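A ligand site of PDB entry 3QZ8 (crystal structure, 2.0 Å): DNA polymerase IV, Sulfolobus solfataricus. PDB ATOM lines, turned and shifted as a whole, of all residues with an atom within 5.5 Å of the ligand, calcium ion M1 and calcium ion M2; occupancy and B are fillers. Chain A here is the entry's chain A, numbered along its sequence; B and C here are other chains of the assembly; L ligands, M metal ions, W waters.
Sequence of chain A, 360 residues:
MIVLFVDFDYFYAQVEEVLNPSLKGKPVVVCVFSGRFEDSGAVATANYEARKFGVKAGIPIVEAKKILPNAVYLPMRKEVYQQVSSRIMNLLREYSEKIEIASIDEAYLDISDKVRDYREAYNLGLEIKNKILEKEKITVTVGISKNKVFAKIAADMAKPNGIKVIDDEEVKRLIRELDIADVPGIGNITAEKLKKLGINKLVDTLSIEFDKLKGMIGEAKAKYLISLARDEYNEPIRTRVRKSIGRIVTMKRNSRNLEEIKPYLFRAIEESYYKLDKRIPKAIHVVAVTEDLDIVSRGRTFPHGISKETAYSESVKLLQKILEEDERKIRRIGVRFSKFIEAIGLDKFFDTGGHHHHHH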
ATOM      1  N   ASP A   7     -22.513  -5.897   5.910  1.00  0.00           N
ATOM      2  CA  ASP A   7     -21.872  -4.645   6.317  1.00  0.00           C
ATOM      3  C   ASP A   7     -22.742  -3.556   5.731  1.00  0.00           C
ATOM      4  O   ASP A   7     -22.917  -3.508   4.532  1.00  0.00           O
ATOM      5  CB  ASP A   7     -20.454  -4.591   5.717  1.00  0.00           C
ATOM      6  CG  ASP A   7     -19.650  -3.349   6.125  1.00  0.00           C
ATOM      7  OD1 ASP A   7     -20.228  -2.341   6.542  1.00  0.00           O
ATOM      8  OD2 ASP A   7     -18.399  -3.408   6.015  1.00  0.00           O
ATOM      9  N   PHE A   8     -23.354  -2.725   6.573  1.00  0.00           N
ATOM     10  CA  PHE A   8     -24.361  -1.762   6.093  1.00  0.00           C
ATOM     11  C   PHE A   8     -23.636  -0.595   5.381  1.00  0.00           C
ATOM     12  O   PHE A   8     -22.548  -0.204   5.819  1.00  0.00           O
ATOM     13  CB  PHE A   8     -25.217  -1.205   7.240  1.00  0.00           C
ATOM     14  CG  PHE A   8     -25.763  -2.248   8.194  1.00  0.00           C
ATOM     15  CD1 PHE A   8     -25.876  -3.577   7.823  1.00  0.00           C
ATOM     16  CD2 PHE A   8     -26.206  -1.864   9.444  1.00  0.00           C
ATOM     17  CE1 PHE A   8     -26.402  -4.525   8.717  1.00  0.00           C
ATOM     18  CE2 PHE A   8     -26.731  -2.806  10.350  1.00  0.00           C
ATOM     19  CZ  PHE A   8     -26.815  -4.143   9.982  1.00  0.00           C
ATOM     20  N   ASP A   9     -24.212  -0.068   4.305  1.00  0.00           N
ATOM     21  CA  ASP A   9     -23.517   0.940   3.481  1.00  0.00           C
ATOM     22  C   ASP A   9     -23.553   2.345   4.100  1.00  0.00           C
ATOM     23  O   ASP A   9     -24.595   2.771   4.573  1.00  0.00           O
ATOM     24  CB  ASP A   9     -24.139   1.023   2.072  1.00  0.00           C
ATOM     25  CG  ASP A   9     -23.971  -0.261   1.249  1.00  0.00           C
ATOM     26  OD1 ASP A   9     -22.956  -0.970   1.411  1.00  0.00           O
ATOM     27  OD2 ASP A   9     -24.872  -0.552   0.426  1.00  0.00           O
ATOM     28  N   TYR A  10     -22.450   3.081   4.038  1.00  0.00           N
ATOM     29  CA  TYR A  10     -22.384   4.436   4.603  1.00  0.00           C
ATOM     30  C   TYR A  10     -23.400   4.653   5.736  1.00  0.00           C
ATOM     31  O   TYR A  10     -24.181   5.595   5.754  1.00  0.00           O
ATOM     32  CB  TYR A  10     -22.499   5.503   3.498  1.00  0.00           C
ATOM     33  CG  TYR A  10     -23.749   5.514   2.649  1.00  0.00           C
ATOM     34  CD1 TYR A  10     -24.682   6.561   2.755  1.00  0.00           C
ATOM     35  CD2 TYR A  10     -24.003   4.517   1.718  1.00  0.00           C
ATOM     36  CE1 TYR A  10     -25.844   6.597   1.951  1.00  0.00           C
ATOM     37  CE2 TYR A  10     -25.171   4.532   0.916  1.00  0.00           C
ATOM     38  CZ  TYR A  10     -26.072   5.586   1.041  1.00  0.00           C
ATOM     39  OH  TYR A  10     -27.214   5.625   0.272  1.00  0.00           O
ATOM     40  N   PHE A  11     -23.316   3.780   6.731  1.00  0.00           N
ATOM     41  CA  PHE A  11     -24.440   3.571   7.614  1.00  0.00           C
ATOM     42  C   PHE A  11     -25.033   4.823   8.241  1.00  0.00           C
ATOM     43  O   PHE A  11     -26.221   5.045   8.085  1.00  0.00           O
ATOM     44  CB  PHE A  11     -24.130   2.524   8.703  1.00  0.00           C
ATOM     45  CG  PHE A  11     -25.327   2.161   9.520  1.00  0.00           C
ATOM     46  CD1 PHE A  11     -26.523   1.791   8.902  1.00  0.00           C
ATOM     47  CD2 PHE A  11     -25.285   2.196  10.909  1.00  0.00           C
ATOM     48  CE1 PHE A  11     -27.658   1.451   9.673  1.00  0.00           C
ATOM     49  CE2 PHE A  11     -26.410   1.854  11.681  1.00  0.00           C
ATOM     50  CZ  PHE A  11     -27.604   1.493  11.066  1.00  0.00           C
ATOM     51  N   TYR A  12     -24.255   5.642   8.958  1.00  0.00           N
ATOM     52  CA  TYR A  12     -24.904   6.749   9.655  1.00  0.00           C
ATOM     53  C   TYR A  12     -25.544   7.675   8.621  1.00  0.00           C
ATOM     54  O   TYR A  12     -26.674   8.133   8.813  1.00  0.00           O
ATOM     55  CB  TYR A  12     -23.944   7.575  10.511  1.00  0.00           C
ATOM     56  CG  TYR A  12     -23.364   6.877  11.742  1.00  0.00           C
ATOM     57  CD1 TYR A  12     -23.692   5.553  12.046  1.00  0.00           C
ATOM     58  CD2 TYR A  12     -22.489   7.553  12.587  1.00  0.00           C
ATOM     59  CE1 TYR A  12     -23.131   4.911  13.144  1.00  0.00           C
ATOM     60  CE2 TYR A  12     -21.915   6.920  13.712  1.00  0.00           C
ATOM     61  CZ  TYR A  12     -22.253   5.591  13.979  1.00  0.00           C
ATOM     62  OH  TYR A  12     -21.727   4.935  15.078  1.00  0.00           O
ATOM     63  N   ALA A  13     -24.838   7.982   7.545  1.00  0.00           N
ATOM     64  CA  ALA A  13     -25.408   8.905   6.553  1.00  0.00           C
ATOM     65  C   ALA A  13     -26.652   8.330   5.899  1.00  0.00           C
ATOM     66  O   ALA A  13     -27.629   9.040   5.624  1.00  0.00           O
ATOM     67  CB  ALA A  13     -24.408   9.265   5.510  1.00  0.00           C
ATOM     68  N   VAL A  43     -15.293  14.148  11.190  1.00  0.00           N
ATOM     69  CA  VAL A  43     -16.317  13.445  10.430  1.00  0.00           C
ATOM     70  C   VAL A  43     -16.463  11.993  10.911  1.00  0.00           C
ATOM     71  O   VAL A  43     -15.467  11.278  11.015  1.00  0.00           O
ATOM     72  CB  VAL A  43     -15.976  13.449   8.935  1.00  0.00           C
ATOM     73  CG1 VAL A  43     -16.956  12.572   8.165  1.00  0.00           C
ATOM     74  CG2 VAL A  43     -15.982  14.870   8.409  1.00  0.00           C
ATOM     75  N   ALA A  44     -17.701  11.554  11.182  1.00  0.00           N
ATOM     76  CA  ALA A  44     -17.978  10.171  11.548  1.00  0.00           C
ATOM     77  C   ALA A  44     -18.088   9.316  10.293  1.00  0.00           C
ATOM     78  O   ALA A  44     -17.483   8.251  10.203  1.00  0.00           O
ATOM     79  CB  ALA A  44     -19.235  10.071  12.383  1.00  0.00           C
ATOM     80  N   THR A  45     -18.882   9.763   9.347  1.00  0.00           N
ATOM     81  CA  THR A  45     -18.873   9.161   8.017  1.00  0.00           C
ATOM     82  C   THR A  45     -19.498  10.149   7.039  1.00  0.00           C
ATOM     83  O   THR A  45     -20.043  11.162   7.452  1.00  0.00           O
ATOM     84  CB  THR A  45     -19.656   7.847   7.951  1.00  0.00           C
ATOM     85  OG1 THR A  45     -19.268   7.144   6.764  1.00  0.00           O
ATOM     86  CG2 THR A  45     -21.169   8.119   7.889  1.00  0.00           C
ATOM     87  N   ALA A  46     -19.389   9.863   5.737  1.00  0.00           N
ATOM     88  CA  ALA A  46     -19.999  10.675   4.690  1.00  0.00           C
ATOM     89  C   ALA A  46     -20.566   9.726   3.651  1.00  0.00           C
ATOM     90  O   ALA A  46     -20.048   8.605   3.507  1.00  0.00           O
ATOM     91  CB  ALA A  46     -18.952  11.565   4.042  1.00  0.00           C
ATOM     92  N   TYR A  48     -21.580   8.479  -0.270  1.00  0.00           N
ATOM     93  CA  TYR A  48     -20.627   8.341  -1.364  1.00  0.00           C
ATOM     94  C   TYR A  48     -20.551   9.619  -2.205  1.00  0.00           C
ATOM     95  O   TYR A  48     -19.538   9.890  -2.827  1.00  0.00           O
ATOM     96  CB  TYR A  48     -20.950   7.090  -2.191  1.00  0.00           C
ATOM     97  CG  TYR A  48     -20.456   5.802  -1.519  1.00  0.00           C
ATOM     98  CD1 TYR A  48     -19.248   5.210  -1.905  1.00  0.00           C
ATOM     99  CD2 TYR A  48     -21.172   5.199  -0.472  1.00  0.00           C
ATOM    100  CE1 TYR A  48     -18.787   4.047  -1.303  1.00  0.00           C
ATOM    101  CE2 TYR A  48     -20.720   4.038   0.130  1.00  0.00           C
ATOM    102  CZ  TYR A  48     -19.528   3.462  -0.286  1.00  0.00           C
ATOM    103  OH  TYR A  48     -19.044   2.299   0.299  1.00  0.00           O
ATOM    104  N   ARG A  51     -17.948  11.421  -0.203  1.00  0.00           N
ATOM    105  CA  ARG A  51     -16.708  10.690  -0.055  1.00  0.00           C
ATOM    106  C   ARG A  51     -15.916  10.714  -1.343  1.00  0.00           C
ATOM    107  O   ARG A  51     -14.694  10.685  -1.340  1.00  0.00           O
ATOM    108  CB  ARG A  51     -17.036   9.244   0.335  1.00  0.00           C
ATOM    109  CG  ARG A  51     -15.902   8.499   0.964  1.00  0.00           C
ATOM    110  CD  ARG A  51     -16.322   7.076   1.272  1.00  0.00           C
ATOM    111  NE  ARG A  51     -17.378   7.021   2.283  1.00  0.00           N
ATOM    112  CZ  ARG A  51     -17.820   5.892   2.817  1.00  0.00           C
ATOM    113  NH1 ARG A  51     -17.292   4.727   2.467  1.00  0.00           N
ATOM    114  NH2 ARG A  51     -18.783   5.925   3.734  1.00  0.00           N
ATOM    115  N   ALA A  57     -14.300   9.580   6.816  1.00  0.00           N
ATOM    116  CA  ALA A  57     -14.292   9.364   8.251  1.00  0.00           C
ATOM    117  C   ALA A  57     -12.966   9.774   8.819  1.00  0.00           C
ATOM    118  O   ALA A  57     -11.910   9.422   8.288  1.00  0.00           O
ATOM    119  CB  ALA A  57     -14.557   7.900   8.559  1.00  0.00           C
ATOM    120  N   GLY A  58     -13.006  10.546   9.903  1.00  0.00           N
ATOM    121  CA  GLY A  58     -11.808  10.871  10.635  1.00  0.00           C
ATOM    122  C   GLY A  58     -11.283  12.266  10.356  1.00  0.00           C
ATOM    123  O   GLY A  58     -10.688  12.877  11.219  1.00  0.00           O
ATOM    124  N   MET A  76     -24.059  13.855  14.601  1.00  0.00           N
ATOM    125  CA  MET A  76     -24.248  12.413  14.800  1.00  0.00           C
ATOM    126  C   MET A  76     -25.410  12.171  15.793  1.00  0.00           C
ATOM    127  O   MET A  76     -25.475  12.804  16.826  1.00  0.00           O
ATOM    128  CB  MET A  76     -22.922  11.805  15.315  1.00  0.00           C
ATOM    129  CG  MET A  76     -22.981  10.320  15.563  1.00  0.00           C
ATOM    130  SD  MET A  76     -21.441   9.679  16.186  1.00  0.00           S
ATOM    131  CE  MET A  76     -21.405  10.361  17.850  1.00  0.00           C
ATOM    132  N   SER A 103     -20.174  -5.140  15.138  1.00  0.00           N
ATOM    133  CA  SER A 103     -20.160  -3.703  15.412  1.00  0.00           C
ATOM    134  C   SER A 103     -21.538  -3.197  15.111  1.00  0.00           C
ATOM    135  O   SER A 103     -22.435  -3.975  14.827  1.00  0.00           O
ATOM    136  CB  SER A 103     -19.153  -2.961  14.546  1.00  0.00           C
ATOM    137  OG  SER A 103     -19.630  -2.903  13.216  1.00  0.00           O
ATOM    138  N   ILE A 104     -21.704  -1.895  15.117  1.00  0.00           N
ATOM    139  CA  ILE A 104     -23.049  -1.351  14.951  1.00  0.00           C
ATOM    140  C   ILE A 104     -23.589  -1.634  13.547  1.00  0.00           C
ATOM    141  O   ILE A 104     -24.799  -1.604  13.332  1.00  0.00           O
ATOM    142  CB  ILE A 104     -23.053   0.165  15.207  1.00  0.00           C
ATOM    143  CG1 ILE A 104     -24.481   0.704  15.197  1.00  0.00           C
ATOM    144  CG2 ILE A 104     -22.195   0.856  14.149  1.00  0.00           C
ATOM    145  CD1 ILE A 104     -24.629   1.999  15.921  1.00  0.00           C
ATOM    146  N   ASP A 105     -22.718  -1.886  12.572  1.00  0.00           N
ATOM    147  CA  ASP A 105     -23.237  -2.118  11.221  1.00  0.00           C
ATOM    148  C   ASP A 105     -22.664  -3.351  10.501  1.00  0.00           C
ATOM    149  O   ASP A 105     -22.668  -3.397   9.286  1.00  0.00           O
ATOM    150  CB  ASP A 105     -23.022  -0.866  10.383  1.00  0.00           C
ATOM    151  CG  ASP A 105     -21.637  -0.818   9.764  1.00  0.00           C
ATOM    152  OD1 ASP A 105     -20.696  -1.247  10.451  1.00  0.00           O
ATOM    153  OD2 ASP A 105     -21.515  -0.386   8.596  1.00  0.00           O
ATOM    154  N   GLU A 106     -22.240  -4.361  11.247  1.00  0.00           N
ATOM    155  CA  GLU A 106     -21.665  -5.563  10.645  1.00  0.00           C
ATOM    156  C   GLU A 106     -22.066  -6.785  11.421  1.00  0.00           C
ATOM    157  O   GLU A 106     -22.118  -6.749  12.645  1.00  0.00           O
ATOM    158  CB  GLU A 106     -20.144  -5.549  10.732  1.00  0.00           C
ATOM    159  CG  GLU A 106     -19.486  -4.365  10.165  1.00  0.00           C
ATOM    160  CD  GLU A 106     -18.013  -4.396  10.486  1.00  0.00           C
ATOM    161  OE1 GLU A 106     -17.680  -4.331  11.685  1.00  0.00           O
ATOM    162  OE2 GLU A 106     -17.206  -4.539   9.560  1.00  0.00           O
ATOM    163  N   LYS A 159     -18.346  -3.481  -2.059  1.00  0.00           N
ATOM    164  CA  LYS A 159     -18.939  -2.229  -1.603  1.00  0.00           C
ATOM    165  C   LYS A 159     -18.988  -1.235  -2.765  1.00  0.00           C
ATOM    166  O   LYS A 159     -18.029  -1.141  -3.522  1.00  0.00           O
ATOM    167  CB  LYS A 159     -18.093  -1.634  -0.471  1.00  0.00           C
ATOM    168  CG  LYS A 159     -18.608  -1.942   0.903  1.00  0.00           C
ATOM    169  CD  LYS A 159     -17.622  -1.448   1.970  1.00  0.00           C
ATOM    170  CE  LYS A 159     -17.946  -2.031   3.353  1.00  0.00           C
ATOM    171  NZ  LYS A 159     -17.269  -1.326   4.518  1.00  0.00           N
ATOM    172  N   PRO A 160     -20.075  -0.474  -2.869  1.00  0.00           N
ATOM    173  CA  PRO A 160     -21.261  -0.503  -2.009  1.00  0.00           C
ATOM    174  C   PRO A 160     -22.425  -1.230  -2.639  1.00  0.00           C
ATOM    175  O   PRO A 160     -22.396  -1.518  -3.825  1.00  0.00           O
ATOM    176  CB  PRO A 160     -21.623   0.970  -1.910  1.00  0.00           C
ATOM    177  CG  PRO A 160     -21.340   1.450  -3.283  1.00  0.00           C
ATOM    178  CD  PRO A 160     -20.098   0.709  -3.736  1.00  0.00           C
ATOM    179  P    DG B   5     -11.357  17.614  18.153  1.00  0.00           P
ATOM    180  OP1  DG B   5     -11.609  18.903  18.848  1.00  0.00           O
ATOM    181  OP2  DG B   5     -10.385  16.607  18.656  1.00  0.00           O
ATOM    182  O5'  DG B   5     -12.785  16.909  18.045  1.00  0.00           O
ATOM    183  C5'  DG B   5     -12.890  15.607  17.514  1.00  0.00           C
ATOM    184  C4'  DG B   5     -14.156  15.023  18.063  1.00  0.00           C
ATOM    185  O4'  DG B   5     -14.546  13.900  17.238  1.00  0.00           O
ATOM    186  C3'  DG B   5     -14.000  14.446  19.472  1.00  0.00           C
ATOM    187  O3'  DG B   5     -15.305  14.455  20.058  1.00  0.00           O
ATOM    188  C2'  DG B   5     -13.429  13.073  19.142  1.00  0.00           C
ATOM    189  C1'  DG B   5     -14.228  12.687  17.896  1.00  0.00           C
ATOM    190  N9   DG B   5     -13.595  11.884  16.853  1.00  0.00           N
ATOM    191  C8   DG B   5     -12.332  11.999  16.345  1.00  0.00           C
ATOM    192  N7   DG B   5     -12.107  11.139  15.388  1.00  0.00           N
ATOM    193  C5   DG B   5     -13.280  10.405  15.236  1.00  0.00           C
ATOM    194  C6   DG B   5     -13.628   9.348  14.355  1.00  0.00           C
ATOM    195  O6   DG B   5     -12.943   8.797  13.482  1.00  0.00           O
ATOM    196  N1   DG B   5     -14.938   8.899  14.558  1.00  0.00           N
ATOM    197  C2   DG B   5     -15.799   9.429  15.492  1.00  0.00           C
ATOM    198  N2   DG B   5     -17.035   8.883  15.555  1.00  0.00           N
ATOM    199  N3   DG B   5     -15.494  10.436  16.306  1.00  0.00           N
ATOM    200  C4   DG B   5     -14.212  10.868  16.135  1.00  0.00           C
ATOM    201  P    DC B   6     -15.500  14.140  21.630  1.00  0.00           P
ATOM    202  OP1  DC B   6     -16.735  14.793  22.076  1.00  0.00           O
ATOM    203  OP2  DC B   6     -14.204  14.321  22.296  1.00  0.00           O
ATOM    204  O5'  DC B   6     -15.767  12.576  21.657  1.00  0.00           O
ATOM    205  C5'  DC B   6     -16.971  12.181  21.050  1.00  0.00           C
ATOM    206  C4'  DC B   6     -16.973  10.675  20.946  1.00  0.00           C
ATOM    207  O4'  DC B   6     -16.171  10.228  19.839  1.00  0.00           O
ATOM    208  C3'  DC B   6     -16.500   9.942  22.224  1.00  0.00           C
ATOM    209  O3'  DC B   6     -17.736   9.368  22.502  1.00  0.00           O
ATOM    210  C2'  DC B   6     -15.392   9.019  21.707  1.00  0.00           C
ATOM    211  C1'  DC B   6     -15.651   8.965  20.202  1.00  0.00           C
ATOM    212  N1   DC B   6     -14.507   8.665  19.307  1.00  0.00           N
ATOM    213  C2   DC B   6     -14.755   7.714  18.340  1.00  0.00           C
ATOM    214  O2   DC B   6     -15.889   7.217  18.319  1.00  0.00           O
ATOM    215  N3   DC B   6     -13.788   7.379  17.458  1.00  0.00           N
ATOM    216  C4   DC B   6     -12.602   7.966  17.551  1.00  0.00           C
ATOM    217  N4   DC B   6     -11.681   7.579  16.665  1.00  0.00           N
ATOM    218  C5   DC B   6     -12.315   8.945  18.534  1.00  0.00           C
ATOM    219  C6   DC B   6     -13.293   9.271  19.390  1.00  0.00           C
ATOM    220  P    DG C  13     -13.543  -1.794   9.885  1.00  0.00           P
ATOM    221  OP1  DG C  13     -13.957  -2.932   9.029  1.00  0.00           O
ATOM    222  OP2  DG C  13     -12.894  -0.619   9.260  1.00  0.00           O
ATOM    223  O5'  DG C  13     -14.795  -1.266  10.723  1.00  0.00           O
ATOM    224  C5'  DG C  13     -15.314  -2.040  11.818  1.00  0.00           C
ATOM    225  C4'  DG C  13     -16.270  -1.175  12.638  1.00  0.00           C
ATOM    226  O4'  DG C  13     -15.452  -0.304  13.477  1.00  0.00           O
ATOM    227  C3'  DG C  13     -17.229  -0.253  11.862  1.00  0.00           C
ATOM    228  O3'  DG C  13     -18.510  -0.190  12.492  1.00  0.00           O
ATOM    229  C2'  DG C  13     -16.561   1.104  11.978  1.00  0.00           C
ATOM    230  C1'  DG C  13     -15.921   1.010  13.375  1.00  0.00           C
ATOM    231  N9   DG C  13     -14.802   1.951  13.515  1.00  0.00           N
ATOM    232  C8   DG C  13     -13.644   2.016  12.780  1.00  0.00           C
ATOM    233  N7   DG C  13     -12.872   2.997  13.168  1.00  0.00           N
ATOM    234  C5   DG C  13     -13.583   3.633  14.184  1.00  0.00           C
ATOM    235  C6   DG C  13     -13.281   4.769  14.978  1.00  0.00           C
ATOM    236  O6   DG C  13     -12.275   5.501  14.964  1.00  0.00           O
ATOM    237  N1   DG C  13     -14.288   5.045  15.897  1.00  0.00           N
ATOM    238  C2   DG C  13     -15.457   4.345  16.025  1.00  0.00           C
ATOM    239  N2   DG C  13     -16.312   4.788  16.951  1.00  0.00           N
ATOM    240  N3   DG C  13     -15.754   3.280  15.299  1.00  0.00           N
ATOM    241  C4   DG C  13     -14.774   2.988  14.413  1.00  0.00           C
HETATM  242  N1  LIG L   1     -17.651   5.263  12.150  1.00  0.00           N
HETATM  243  C1  LIG L   1     -17.128   6.307  13.001  1.00  0.00           C
HETATM  244  N2  LIG L   1     -15.759   6.700  12.928  1.00  0.00           N
HETATM  245  C2  LIG L   1     -14.877   6.062  12.003  1.00  0.00           C
HETATM  246  C3  LIG L   1     -15.371   5.001  11.118  1.00  0.00           C
HETATM  247  C4  LIG L   1     -16.798   4.630  11.201  1.00  0.00           C
HETATM  248  O1  LIG L   1     -17.840   6.864  13.819  1.00  0.00           O
HETATM  249  N3  LIG L   1     -13.512   6.484  11.971  1.00  0.00           N
HETATM  250  C5  LIG L   1     -19.071   4.913  12.231  1.00  0.00           C
HETATM  251  C6  LIG L   1     -19.859   5.615  11.192  1.00  0.00           C
HETATM  252  C7  LIG L   1     -19.983   4.637  10.095  1.00  0.00           C
HETATM  253  C8  LIG L   1     -20.052   3.352  10.775  1.00  0.00           C
HETATM  254  O2  LIG L   1     -19.304   3.563  12.026  1.00  0.00           O
HETATM  255  O3  LIG L   1     -21.135   4.901   9.350  1.00  0.00           O
HETATM  256  C9  LIG L   1     -19.557   2.184   9.915  1.00  0.00           C
HETATM  257  O4  LIG L   1     -18.226   2.140   9.427  1.00  0.00           O
HETATM  258  P1  LIG L   1     -17.809   1.760   7.928  1.00  0.00           P
HETATM  259  O5  LIG L   1     -16.403   1.773   8.553  1.00  0.00           O
HETATM  260  O6  LIG L   1     -18.657   0.494   7.955  1.00  0.00           O
HETATM  261  O7  LIG L   1     -18.459   3.094   7.301  1.00  0.00           O
HETATM  262  P2  LIG L   1     -19.753   3.295   6.362  1.00  0.00           P
HETATM  263  O8  LIG L   1     -20.563   2.121   6.896  1.00  0.00           O
HETATM  264  O9  LIG L   1     -19.827   4.717   6.991  1.00  0.00           O
HETATM  265  O10 LIG L   1     -18.942   3.160   5.043  1.00  0.00           O
HETATM  266  P3  LIG L   1     -18.978   1.935   4.068  1.00  0.00           P
HETATM  267  O11 LIG L   1     -19.066   0.680   4.882  1.00  0.00           O
HETATM  268  O12 LIG L   1     -17.611   2.022   3.417  1.00  0.00           O
HETATM  269  O13 LIG L   1     -20.110   1.960   3.072  1.00  0.00           O
HETATM  270 CA    CA M   1     -20.454  -0.080   6.624  1.00  0.00          CA
HETATM  271 CA    CA M   2     -18.611  -1.651   9.007  1.00  0.00          CA
HETATM  272  O   HOH W   1     -11.746   5.520  10.197  1.00  0.00           O
HETATM  273  O   HOH W   2     -18.869   2.218  14.991  1.00  0.00           O
HETATM  274  O   HOH W   3     -19.507   6.137  16.040  1.00  0.00           O
HETATM  275  O   HOH W   4     -16.594  -2.641   7.981  1.00  0.00           O
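Calcium ion M1 is bound by an oxygen (O8) of the ligand (2.2 Å), the backbone carbonyl oxygen (O) of Phe 8 (2.2 Å), the side-chain carboxylate (OD2) of Asp 105 (2.3 Å), the side-chain carboxylate (OD1) of Asp 7 (2.3 Å), an oxygen (O6) of the ligand (2.3 Å) and an oxygen (O11) of the ligand (2.4 Å). Calcium ion M1 has six donor atoms within binding distance.
Asp 9 touches the ligand. Ala 44 touches the ligand (O to C1, 3.4 Å). CB of Ala 57 touches N3 of the ligand, at 3.8 Å. Hydrophobic or aromatic side chains that line the ligand: Phe 11, Tyr 12, Ala 44, Tyr 48 and Ala 57. The nearest printed residue that does not touch the ligand is Ile 104 (4.5 Å).
Three residues have an atom within 4 Å of calcium ion M1: Asp 7, Phe 8 and Asp 105. The nearest printed residue that does not touch calcium ion M1 is Lys 159 (4.02 Å).
Calcium ion M2 is bound by an oxygen (O6) of the ligand (2.4 Å), water W4 (2.5 Å) and the side-chain carboxylate (OD1) of Asp 105 (2.6 Å). Calcium ion M2 has three donor atoms within binding distance. Slightly farther from calcium ion M2 lies OD1 of Asp 7 (3.0 Å).
The side-chain carboxylate (OE1) of Glu 106 is in hydrogen-bond range of the side-chain hydroxyl (OG) of Ser 103, 2.9 Å away. The side-chain amino group (NZ) of Lys 159 is in salt-bridge range of the side-chain carboxylate (OD2) of Asp 7, at 2.8 Å. The guanidinium group of Arg 51 lies within hydrogen-bond range of the side-chain hydroxyl of Thr 45, at 3.3 Å. The side-chain hydroxyl of Ser 103 sits at hydrogen-bond distance from O3' of DG 13 of chain C, 3.0 Å away. N of Asp 105 sits close to OG of Ser 103 (3.3 Å). N4 of DC 6 of chain B lies close to O6 of DG 13 of chain C, at 2.8 Å. O of Ala 46 sits at hydrogen-bond distance from NH2 of Arg 51 (3.0 Å).
O6 of DG 13 of chain C is in hydrogen-bond range of N3 of the ligand (3.4 Å). The backbone NH of Phe 11 sits close to an oxygen (O8) of the ligand (3.2 Å). O6 of DG 5 of chain B lies within hydrogen-bond range of a nitrogen (N3) of the ligand, 2.8 Å away. The side-chain amino group of Lys 159 is in salt-bridge range of an oxygen (O12) of the ligand (3.5 Å). O12 of the ligand lies within salt-bridge range of NH1 of Arg 51 (2.9 Å). OG1 of Thr 45 is in hydrogen-bond range of O9 of the ligand (2.5 Å). OH of Tyr 48 sits at hydrogen-bond distance from O13 of the ligand (3.0 Å). The backbone NH (N) of Tyr 12 is in hydrogen-bond range of an oxygen (O3) of the ligand (3.2 Å). An oxygen (O13) of the ligand is in hydrogen-bond range of the backbone NH of Tyr 10 (2.8 Å).
Water W3 bridges OH of Tyr 12 (2.7 Å) and O1 of the ligand (2.9 Å). Water W2 bridges an oxygen (O2) of the ligand (3.3 Å) and N3 of DG 13 of chain C (3.3 Å).
Residues that only touch calcium ion M2: Glu 106 (3.1 Å) and DG 13 of chain C (3.5 Å). Within 4 Å of calcium ion M2: Asp 7, Asp 105, Glu 106 and DG 13 of chain C.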
